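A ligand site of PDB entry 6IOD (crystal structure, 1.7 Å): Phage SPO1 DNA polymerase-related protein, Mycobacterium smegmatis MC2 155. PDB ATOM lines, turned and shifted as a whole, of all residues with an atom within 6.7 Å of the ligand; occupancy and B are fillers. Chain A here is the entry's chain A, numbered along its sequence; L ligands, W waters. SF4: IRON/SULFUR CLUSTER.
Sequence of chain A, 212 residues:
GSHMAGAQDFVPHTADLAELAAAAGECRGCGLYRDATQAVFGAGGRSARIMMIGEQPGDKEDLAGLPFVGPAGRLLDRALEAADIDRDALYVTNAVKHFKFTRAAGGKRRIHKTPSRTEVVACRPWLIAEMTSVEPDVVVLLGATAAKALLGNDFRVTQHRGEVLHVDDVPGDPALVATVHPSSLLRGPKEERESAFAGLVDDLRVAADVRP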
ATOM      1  N   GLY A   6       5.354 -12.897  13.642  1.00  0.00           N
ATOM      2  CA  GLY A   6       5.060 -12.405  12.312  1.00  0.00           C
ATOM      3  C   GLY A   6       5.556 -10.988  12.106  1.00  0.00           C
ATOM      4  O   GLY A   6       5.772 -10.216  13.050  1.00  0.00           O
ATOM      5  N   ALA A   7       5.731 -10.646  10.817  1.00  0.00           N
ATOM      6  CA  ALA A   7       6.308  -9.363  10.441  1.00  0.00           C
ATOM      7  C   ALA A   7       5.286  -8.229  10.385  1.00  0.00           C
ATOM      8  O   ALA A   7       5.699  -7.082  10.251  1.00  0.00           O
ATOM      9  CB  ALA A   7       6.982  -9.458   9.056  1.00  0.00           C
ATOM     10  N   PHE A  10       5.798  -4.875  11.995  1.00  0.00           N
ATOM     11  CA  PHE A  10       7.053  -4.222  11.683  1.00  0.00           C
ATOM     12  C   PHE A  10       7.039  -3.535  10.323  1.00  0.00           C
ATOM     13  O   PHE A  10       7.995  -2.824  10.009  1.00  0.00           O
ATOM     14  CB  PHE A  10       8.199  -5.238  11.694  1.00  0.00           C
ATOM     15  CG  PHE A  10       8.539  -5.782  13.070  1.00  0.00           C
ATOM     16  CD1 PHE A  10       9.410  -5.095  13.899  1.00  0.00           C
ATOM     17  CD2 PHE A  10       8.004  -6.984  13.502  1.00  0.00           C
ATOM     18  CE1 PHE A  10       9.766  -5.601  15.164  1.00  0.00           C
ATOM     19  CE2 PHE A  10       8.362  -7.491  14.789  1.00  0.00           C
ATOM     20  CZ  PHE A  10       9.198  -6.774  15.601  1.00  0.00           C
ATOM     21  N   ALA A  24      12.762  -3.550   7.137  1.00  0.00           N
ATOM     22  CA  ALA A  24      13.011  -4.984   7.249  1.00  0.00           C
ATOM     23  C   ALA A  24      14.306  -5.276   7.993  1.00  0.00           C
ATOM     24  O   ALA A  24      14.425  -6.299   8.664  1.00  0.00           O
ATOM     25  CB  ALA A  24      13.029  -5.664   5.870  1.00  0.00           C
ATOM     26  N   GLY A  25      15.281  -4.359   7.945  1.00  0.00           N
ATOM     27  CA  GLY A  25      16.480  -4.582   8.721  1.00  0.00           C
ATOM     28  C   GLY A  25      16.244  -4.518  10.216  1.00  0.00           C
ATOM     29  O   GLY A  25      17.129  -4.895  10.993  1.00  0.00           O
ATOM     30  N   GLU A  26      15.083  -4.030  10.636  1.00  0.00           N
ATOM     31  CA  GLU A  26      14.737  -3.977  12.050  1.00  0.00           C
ATOM     32  C   GLU A  26      13.681  -4.998  12.430  1.00  0.00           C
ATOM     33  O   GLU A  26      13.229  -5.024  13.577  1.00  0.00           O
ATOM     34  CB  GLU A  26      14.216  -2.590  12.416  1.00  0.00           C
ATOM     35  CG  GLU A  26      15.225  -1.504  12.220  1.00  0.00           C
ATOM     36  CD  GLU A  26      14.770  -0.252  12.903  1.00  0.00           C
ATOM     37  OE1 GLU A  26      13.679   0.245  12.562  1.00  0.00           O
ATOM     38  OE2 GLU A  26      15.491   0.194  13.822  1.00  0.00           O
ATOM     39  N   CYS A  27      13.277  -5.831  11.479  1.00  0.00           N
ATOM     40  CA  CYS A  27      12.215  -6.793  11.716  1.00  0.00           C
ATOM     41  C   CYS A  27      12.663  -7.888  12.677  1.00  0.00           C
ATOM     42  O   CYS A  27      13.799  -8.357  12.630  1.00  0.00           O
ATOM     43  CB  CYS A  27      11.780  -7.416  10.387  1.00  0.00           C
ATOM     44  SG  CYS A  27      10.387  -8.542  10.526  1.00  0.00           S
ATOM     45  N   ARG A  28      11.742  -8.277  13.575  1.00  0.00           N
ATOM     46  CA  ARG A  28      11.916  -9.400  14.476  1.00  0.00           C
ATOM     47  C   ARG A  28      10.685 -10.296  14.426  1.00  0.00           C
ATOM     48  O   ARG A  28      10.260 -10.871  15.444  1.00  0.00           O
ATOM     49  CB  ARG A  28      12.176  -8.931  15.920  1.00  0.00           C
ATOM     50  CG  ARG A  28      13.396  -8.040  16.044  1.00  0.00           C
ATOM     51  CD  ARG A  28      13.638  -7.516  17.448  1.00  0.00           C
ATOM     52  NE  ARG A  28      14.990  -6.987  17.471  1.00  0.00           N
ATOM     53  CZ  ARG A  28      15.936  -7.323  18.340  1.00  0.00           C
ATOM     54  NH1 ARG A  28      15.667  -8.175  19.329  1.00  0.00           N
ATOM     55  NH2 ARG A  28      17.149  -6.779  18.213  1.00  0.00           N
ATOM     56  N   GLY A  29      10.097 -10.420  13.223  1.00  0.00           N
ATOM     57  CA  GLY A  29       8.886 -11.201  13.045  1.00  0.00           C
ATOM     58  C   GLY A  29       9.081 -12.682  13.184  1.00  0.00           C
ATOM     59  O   GLY A  29       8.119 -13.439  13.401  1.00  0.00           O
ATOM     60  N   CYS A  30      10.310 -13.150  13.035  1.00  0.00           N
ATOM     61  CA  CYS A  30      10.597 -14.525  13.346  1.00  0.00           C
ATOM     62  C   CYS A  30      12.008 -14.573  13.905  1.00  0.00           C
ATOM     63  O   CYS A  30      12.619 -13.532  14.162  1.00  0.00           O
ATOM     64  CB  CYS A  30      10.394 -15.437  12.129  1.00  0.00           C
ATOM     65  SG  CYS A  30      11.654 -15.350  10.813  1.00  0.00           S
ATOM     66  N   GLY A  31      12.529 -15.780  14.115  1.00  0.00           N
ATOM     67  CA  GLY A  31      13.844 -15.852  14.717  1.00  0.00           C
ATOM     68  C   GLY A  31      15.011 -15.646  13.772  1.00  0.00           C
ATOM     69  O   GLY A  31      16.162 -15.565  14.228  1.00  0.00           O
ATOM     70  N   LEU A  32      14.741 -15.543  12.456  1.00  0.00           N
ATOM     71  CA  LEU A  32      15.854 -15.620  11.500  1.00  0.00           C
ATOM     72  C   LEU A  32      16.734 -14.373  11.506  1.00  0.00           C
ATOM     73  O   LEU A  32      17.884 -14.445  11.060  1.00  0.00           O
ATOM     74  CB  LEU A  32      15.319 -15.868  10.085  1.00  0.00           C
ATOM     75  CG  LEU A  32      14.577 -17.206   9.926  1.00  0.00           C
ATOM     76  CD1 LEU A  32      14.088 -17.388   8.477  1.00  0.00           C
ATOM     77  CD2 LEU A  32      15.498 -18.360  10.300  1.00  0.00           C
ATOM     78  N   TYR A  33      16.247 -13.238  11.995  1.00  0.00           N
ATOM     79  CA  TYR A  33      17.085 -12.047  12.046  1.00  0.00           C
ATOM     80  C   TYR A  33      18.319 -12.248  12.932  1.00  0.00           C
ATOM     81  O   TYR A  33      19.331 -11.572  12.728  1.00  0.00           O
ATOM     82  CB  TYR A  33      16.280 -10.850  12.547  1.00  0.00           C
ATOM     83  CG  TYR A  33      16.017 -10.935  14.038  1.00  0.00           C
ATOM     84  CD1 TYR A  33      14.927 -11.624  14.522  1.00  0.00           C
ATOM     85  CD2 TYR A  33      16.876 -10.331  14.948  1.00  0.00           C
ATOM     86  CE1 TYR A  33      14.686 -11.739  15.888  1.00  0.00           C
ATOM     87  CE2 TYR A  33      16.639 -10.435  16.323  1.00  0.00           C
ATOM     88  CZ  TYR A  33      15.539 -11.129  16.763  1.00  0.00           C
ATOM     89  OH  TYR A  33      15.283 -11.246  18.125  1.00  0.00           O
ATOM     90  N   ARG A  34      18.265 -13.177  13.894  1.00  0.00           N
ATOM     91  CA  ARG A  34      19.301 -13.224  14.912  1.00  0.00           C
ATOM     92  C   ARG A  34      20.636 -13.675  14.341  1.00  0.00           C
ATOM     93  O   ARG A  34      21.661 -12.999  14.545  1.00  0.00           O
ATOM     94  CB  ARG A  34      18.884 -14.120  16.072  1.00  0.00           C
ATOM     95  CG  ARG A  34      17.838 -13.483  16.980  1.00  0.00           C
ATOM     96  CD  ARG A  34      17.651 -14.301  18.239  1.00  0.00           C
ATOM     97  NE  ARG A  34      17.192 -15.642  17.894  1.00  0.00           N
ATOM     98  CZ  ARG A  34      15.923 -16.032  17.916  1.00  0.00           C
ATOM     99  NH1 ARG A  34      14.958 -15.186  18.274  1.00  0.00           N
ATOM    100  NH2 ARG A  34      15.635 -17.284  17.577  1.00  0.00           N
ATOM    101  N   ALA A  39      19.232  -8.180   6.652  1.00  0.00           N
ATOM    102  CA  ALA A  39      18.080  -8.495   5.815  1.00  0.00           C
ATOM    103  C   ALA A  39      18.473  -8.378   4.343  1.00  0.00           C
ATOM    104  O   ALA A  39      19.297  -7.541   3.972  1.00  0.00           O
ATOM    105  CB  ALA A  39      16.907  -7.563   6.116  1.00  0.00           C
ATOM    106  N   ALA A  95      10.877 -14.997  -0.692  1.00  0.00           N
ATOM    107  CA  ALA A  95       9.761 -15.115   0.246  1.00  0.00           C
ATOM    108  C   ALA A  95      10.179 -14.819   1.669  1.00  0.00           C
ATOM    109  O   ALA A  95       9.369 -14.330   2.464  1.00  0.00           O
ATOM    110  CB  ALA A  95       9.129 -16.506   0.141  1.00  0.00           C
ATOM    111  N   VAL A  96      11.442 -15.109   2.020  1.00  0.00           N
ATOM    112  CA  VAL A  96      11.970 -14.946   3.356  1.00  0.00           C
ATOM    113  C   VAL A  96      13.211 -14.072   3.234  1.00  0.00           C
ATOM    114  O   VAL A  96      14.007 -14.247   2.296  1.00  0.00           O
ATOM    115  CB  VAL A  96      12.261 -16.326   3.968  1.00  0.00           C
ATOM    116  CG1 VAL A  96      13.157 -16.240   5.192  1.00  0.00           C
ATOM    117  CG2 VAL A  96      10.908 -17.001   4.300  1.00  0.00           C
ATOM    118  N   LYS A  97      13.353 -13.080   4.137  1.00  0.00           N
ATOM    119  CA  LYS A  97      14.318 -11.983   4.022  1.00  0.00           C
ATOM    120  C   LYS A  97      15.604 -12.176   4.815  1.00  0.00           C
ATOM    121  O   LYS A  97      16.546 -11.414   4.591  1.00  0.00           O
ATOM    122  CB  LYS A  97      13.677 -10.677   4.491  1.00  0.00           C
ATOM    123  CG  LYS A  97      13.102  -9.749   3.468  1.00  0.00           C
ATOM    124  CD  LYS A  97      12.211 -10.432   2.483  1.00  0.00           C
ATOM    125  CE  LYS A  97      11.471  -9.404   1.572  1.00  0.00           C
ATOM    126  NZ  LYS A  97      10.536 -10.180   0.660  1.00  0.00           N
ATOM    127  N   HIS A  98      15.690 -13.159   5.711  1.00  0.00           N
ATOM    128  CA  HIS A  98      16.915 -13.391   6.475  1.00  0.00           C
ATOM    129  C   HIS A  98      17.377 -14.821   6.241  1.00  0.00           C
ATOM    130  O   HIS A  98      16.556 -15.738   6.205  1.00  0.00           O
ATOM    131  CB  HIS A  98      16.693 -13.168   7.990  1.00  0.00           C
ATOM    132  CG  HIS A  98      16.695 -11.740   8.420  1.00  0.00           C
ATOM    133  ND1 HIS A  98      15.555 -11.046   8.754  1.00  0.00           N
ATOM    134  CD2 HIS A  98      17.718 -10.878   8.579  1.00  0.00           C
ATOM    135  CE1 HIS A  98      15.873  -9.808   9.094  1.00  0.00           C
ATOM    136  NE2 HIS A  98      17.186  -9.690   9.022  1.00  0.00           N
ATOM    137  N   PHE A  99      18.689 -14.992   6.066  1.00  0.00           N
ATOM    138  CA  PHE A  99      19.295 -16.296   5.758  1.00  0.00           C
ATOM    139  C   PHE A  99      19.154 -17.284   6.911  1.00  0.00           C
ATOM    140  O   PHE A  99      19.684 -17.057   8.009  1.00  0.00           O
ATOM    141  CB  PHE A  99      20.765 -16.048   5.390  1.00  0.00           C
ATOM    142  CG  PHE A  99      21.556 -17.273   5.040  1.00  0.00           C
ATOM    143  CD1 PHE A  99      21.033 -18.283   4.226  1.00  0.00           C
ATOM    144  CD2 PHE A  99      22.865 -17.379   5.478  1.00  0.00           C
ATOM    145  CE1 PHE A  99      21.802 -19.383   3.883  1.00  0.00           C
ATOM    146  CE2 PHE A  99      23.650 -18.479   5.129  1.00  0.00           C
ATOM    147  CZ  PHE A  99      23.140 -19.473   4.346  1.00  0.00           C
ATOM    148  N   GLU A 119       7.978 -19.699   9.088  1.00  0.00           N
ATOM    149  CA  GLU A 119       8.779 -18.515   8.768  1.00  0.00           C
ATOM    150  C   GLU A 119       8.297 -17.850   7.493  1.00  0.00           C
ATOM    151  O   GLU A 119       8.293 -16.611   7.401  1.00  0.00           O
ATOM    152  CB  GLU A 119      10.279 -18.900   8.697  1.00  0.00           C
ATOM    153  CG  GLU A 119      10.823 -19.302  10.075  1.00  0.00           C
ATOM    154  CD  GLU A 119      12.008 -20.246  10.016  1.00  0.00           C
ATOM    155  OE1 GLU A 119      12.204 -20.895   8.989  1.00  0.00           O
ATOM    156  OE2 GLU A 119      12.648 -20.467  11.080  1.00  0.00           O
ATOM    157  N   ALA A 122       5.354 -15.898   8.416  1.00  0.00           N
ATOM    158  CA  ALA A 122       5.776 -14.764   9.226  1.00  0.00           C
ATOM    159  C   ALA A 122       6.308 -13.650   8.355  1.00  0.00           C
ATOM    160  O   ALA A 122       6.015 -12.469   8.611  1.00  0.00           O
ATOM    161  CB  ALA A 122       6.846 -15.180  10.245  1.00  0.00           C
ATOM    162  N   CYS A 123       7.063 -14.000   7.309  1.00  0.00           N
ATOM    163  CA  CYS A 123       7.712 -12.986   6.485  1.00  0.00           C
ATOM    164  C   CYS A 123       6.805 -12.446   5.375  1.00  0.00           C
ATOM    165  O   CYS A 123       7.127 -11.404   4.783  1.00  0.00           O
ATOM    166  CB  CYS A 123       9.006 -13.561   5.867  1.00  0.00           C
ATOM    167  SG  CYS A 123      10.241 -12.299   5.513  1.00  0.00           S
ATOM    168  N   ARG A 124       5.705 -13.136   5.100  1.00  0.00           N
ATOM    169  CA  ARG A 124       4.902 -12.803   3.931  1.00  0.00           C
ATOM    170  C   ARG A 124       4.434 -11.353   3.924  1.00  0.00           C
ATOM    171  O   ARG A 124       4.274 -10.805   2.821  1.00  0.00           O
ATOM    172  CB  ARG A 124       3.723 -13.768   3.826  1.00  0.00           C
ATOM    173  CG  ARG A 124       2.985 -13.634   2.520  1.00  0.00           C
ATOM    174  CD  ARG A 124       2.066 -14.820   2.328  1.00  0.00           C
ATOM    175  NE  ARG A 124       1.148 -14.910   3.454  1.00  0.00           N
ATOM    176  CZ  ARG A 124       0.438 -15.988   3.743  1.00  0.00           C
ATOM    177  NH1 ARG A 124       0.557 -17.071   2.978  1.00  0.00           N
ATOM    178  NH2 ARG A 124      -0.377 -16.007   4.785  1.00  0.00           N
ATOM    179  N   PRO A 125       4.209 -10.679   5.054  1.00  0.00           N
ATOM    180  CA  PRO A 125       3.761  -9.273   4.957  1.00  0.00           C
ATOM    181  C   PRO A 125       4.719  -8.391   4.188  1.00  0.00           C
ATOM    182  O   PRO A 125       4.283  -7.426   3.548  1.00  0.00           O
ATOM    183  CB  PRO A 125       3.673  -8.836   6.427  1.00  0.00           C
ATOM    184  CG  PRO A 125       3.203 -10.120   7.131  1.00  0.00           C
ATOM    185  CD  PRO A 125       4.010 -11.211   6.435  1.00  0.00           C
ATOM    186  N   TRP A 126       6.026  -8.678   4.252  1.00  0.00           N
ATOM    187  CA  TRP A 126       6.955  -7.916   3.418  1.00  0.00           C
ATOM    188  C   TRP A 126       6.684  -8.126   1.931  1.00  0.00           C
ATOM    189  O   TRP A 126       6.719  -7.167   1.148  1.00  0.00           O
ATOM    190  CB  TRP A 126       8.411  -8.290   3.747  1.00  0.00           C
ATOM    191  CG  TRP A 126       8.845  -7.877   5.137  1.00  0.00           C
ATOM    192  CD1 TRP A 126       9.162  -8.703   6.179  1.00  0.00           C
ATOM    193  CD2 TRP A 126       8.989  -6.543   5.629  1.00  0.00           C
ATOM    194  NE1 TRP A 126       9.506  -7.963   7.294  1.00  0.00           N
ATOM    195  CE2 TRP A 126       9.387  -6.625   6.976  1.00  0.00           C
ATOM    196  CE3 TRP A 126       8.818  -5.279   5.057  1.00  0.00           C
ATOM    197  CZ2 TRP A 126       9.626  -5.492   7.755  1.00  0.00           C
ATOM    198  CZ3 TRP A 126       9.048  -4.151   5.846  1.00  0.00           C
ATOM    199  CH2 TRP A 126       9.439  -4.266   7.178  1.00  0.00           C
HETATM  200 FE1  SF4 L   1      11.719 -13.247   9.928  1.00  0.00          FE
HETATM  201 FE2  SF4 L   1      13.562 -11.634   8.852  1.00  0.00          FE
HETATM  202 FE3  SF4 L   1      11.332 -10.578   9.762  1.00  0.00          FE
HETATM  203 FE4  SF4 L   1      11.285 -12.054   7.551  1.00  0.00          FE
HETATM  204  S1  SF4 L   1      12.320 -10.086   7.782  1.00  0.00           S
HETATM  205  S2  SF4 L   1       9.861 -12.200   9.304  1.00  0.00           S
HETATM  206  S3  SF4 L   1      12.870 -13.537   7.999  1.00  0.00           S
HETATM  207  S4  SF4 L   1      12.846 -11.663  11.001  1.00  0.00           S
HETATM  208  O   HOH W   1      11.156 -15.872   7.683  1.00  0.00           O
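Merely in contact with the ligand: Lys 97 (3.6 Å), Tyr 33 (3.9 Å), Val 96 (3.9 Å), Ala 122 (3.9 Å), Leu 32 (3.97 Å) and Ala 7 (3.98 Å).
Hydrophobic or aromatic side chains within 4 Å of the ligand: Ala 7, Leu 32, Tyr 33, Val 96, His 98 and Trp 126.
Within 4 Å of the ligand: Ala 7, Cys 27, Gly 29, Cys 30, Leu 32, Tyr 33, Val 96, Lys 97, His 98, Ala 122, Cys 123 and Trp 126.
The nearest printed residue that does not touch the ligand is Arg 28 (4.2 Å).
Water W1 bridges a sulfur (S3) of the ligand and the backbone carbonyl oxygen of Glu 119.
N of Cys 30 lies close to S4 of the ligand, at 3.6 Å.
NE1 of Trp 126 sits close to S1 of the ligand.
An iron atom (FE2) of the ligand is bound by a ring nitrogen (ND1) of His 98.
The backbone NH of Gly 29 sits close to a sulfur (S4) of the ligand, 3.7 Å away.
FE1 of the ligand is bound by SG of Cys 30.
An iron atom (FE4) of the ligand is bound by the side-chain sulfur (SG) of Cys 123.
FE3 of the ligand is bound by SG of Cys 27 (2.4 Å).
N of His 98 sits close to S3 of the ligand, at 3.7 Å.
N of Ala 39 is in hydrogen-bond range of NE2 of His 98, 3.5 Å away.
O of Ala 95 lies close to SG of Cys 123 (3.8 Å).
The side-chain sulfur of Cys 27 sits close to the indole nitrogen of Trp 126, at 3.4 Å.
N of Leu 32 lies close to SG of Cys 30 (3.5 Å).
The backbone carbonyl oxygen of Gly 29 lies within hydrogen-bond range of the backbone NH of Gly 6 (2.8 Å).
The side-chain sulfur (SG) of Cys 27 lies close to the backbone NH (N) of Gly 29 (3.3 Å).
The backbone NH (N) of Lys 97 lies close to the side-chain sulfur (SG) of Cys 123, 3.5 Å away.
OH of Tyr 33 is in hydrogen-bond range of NH1 of Arg 28.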
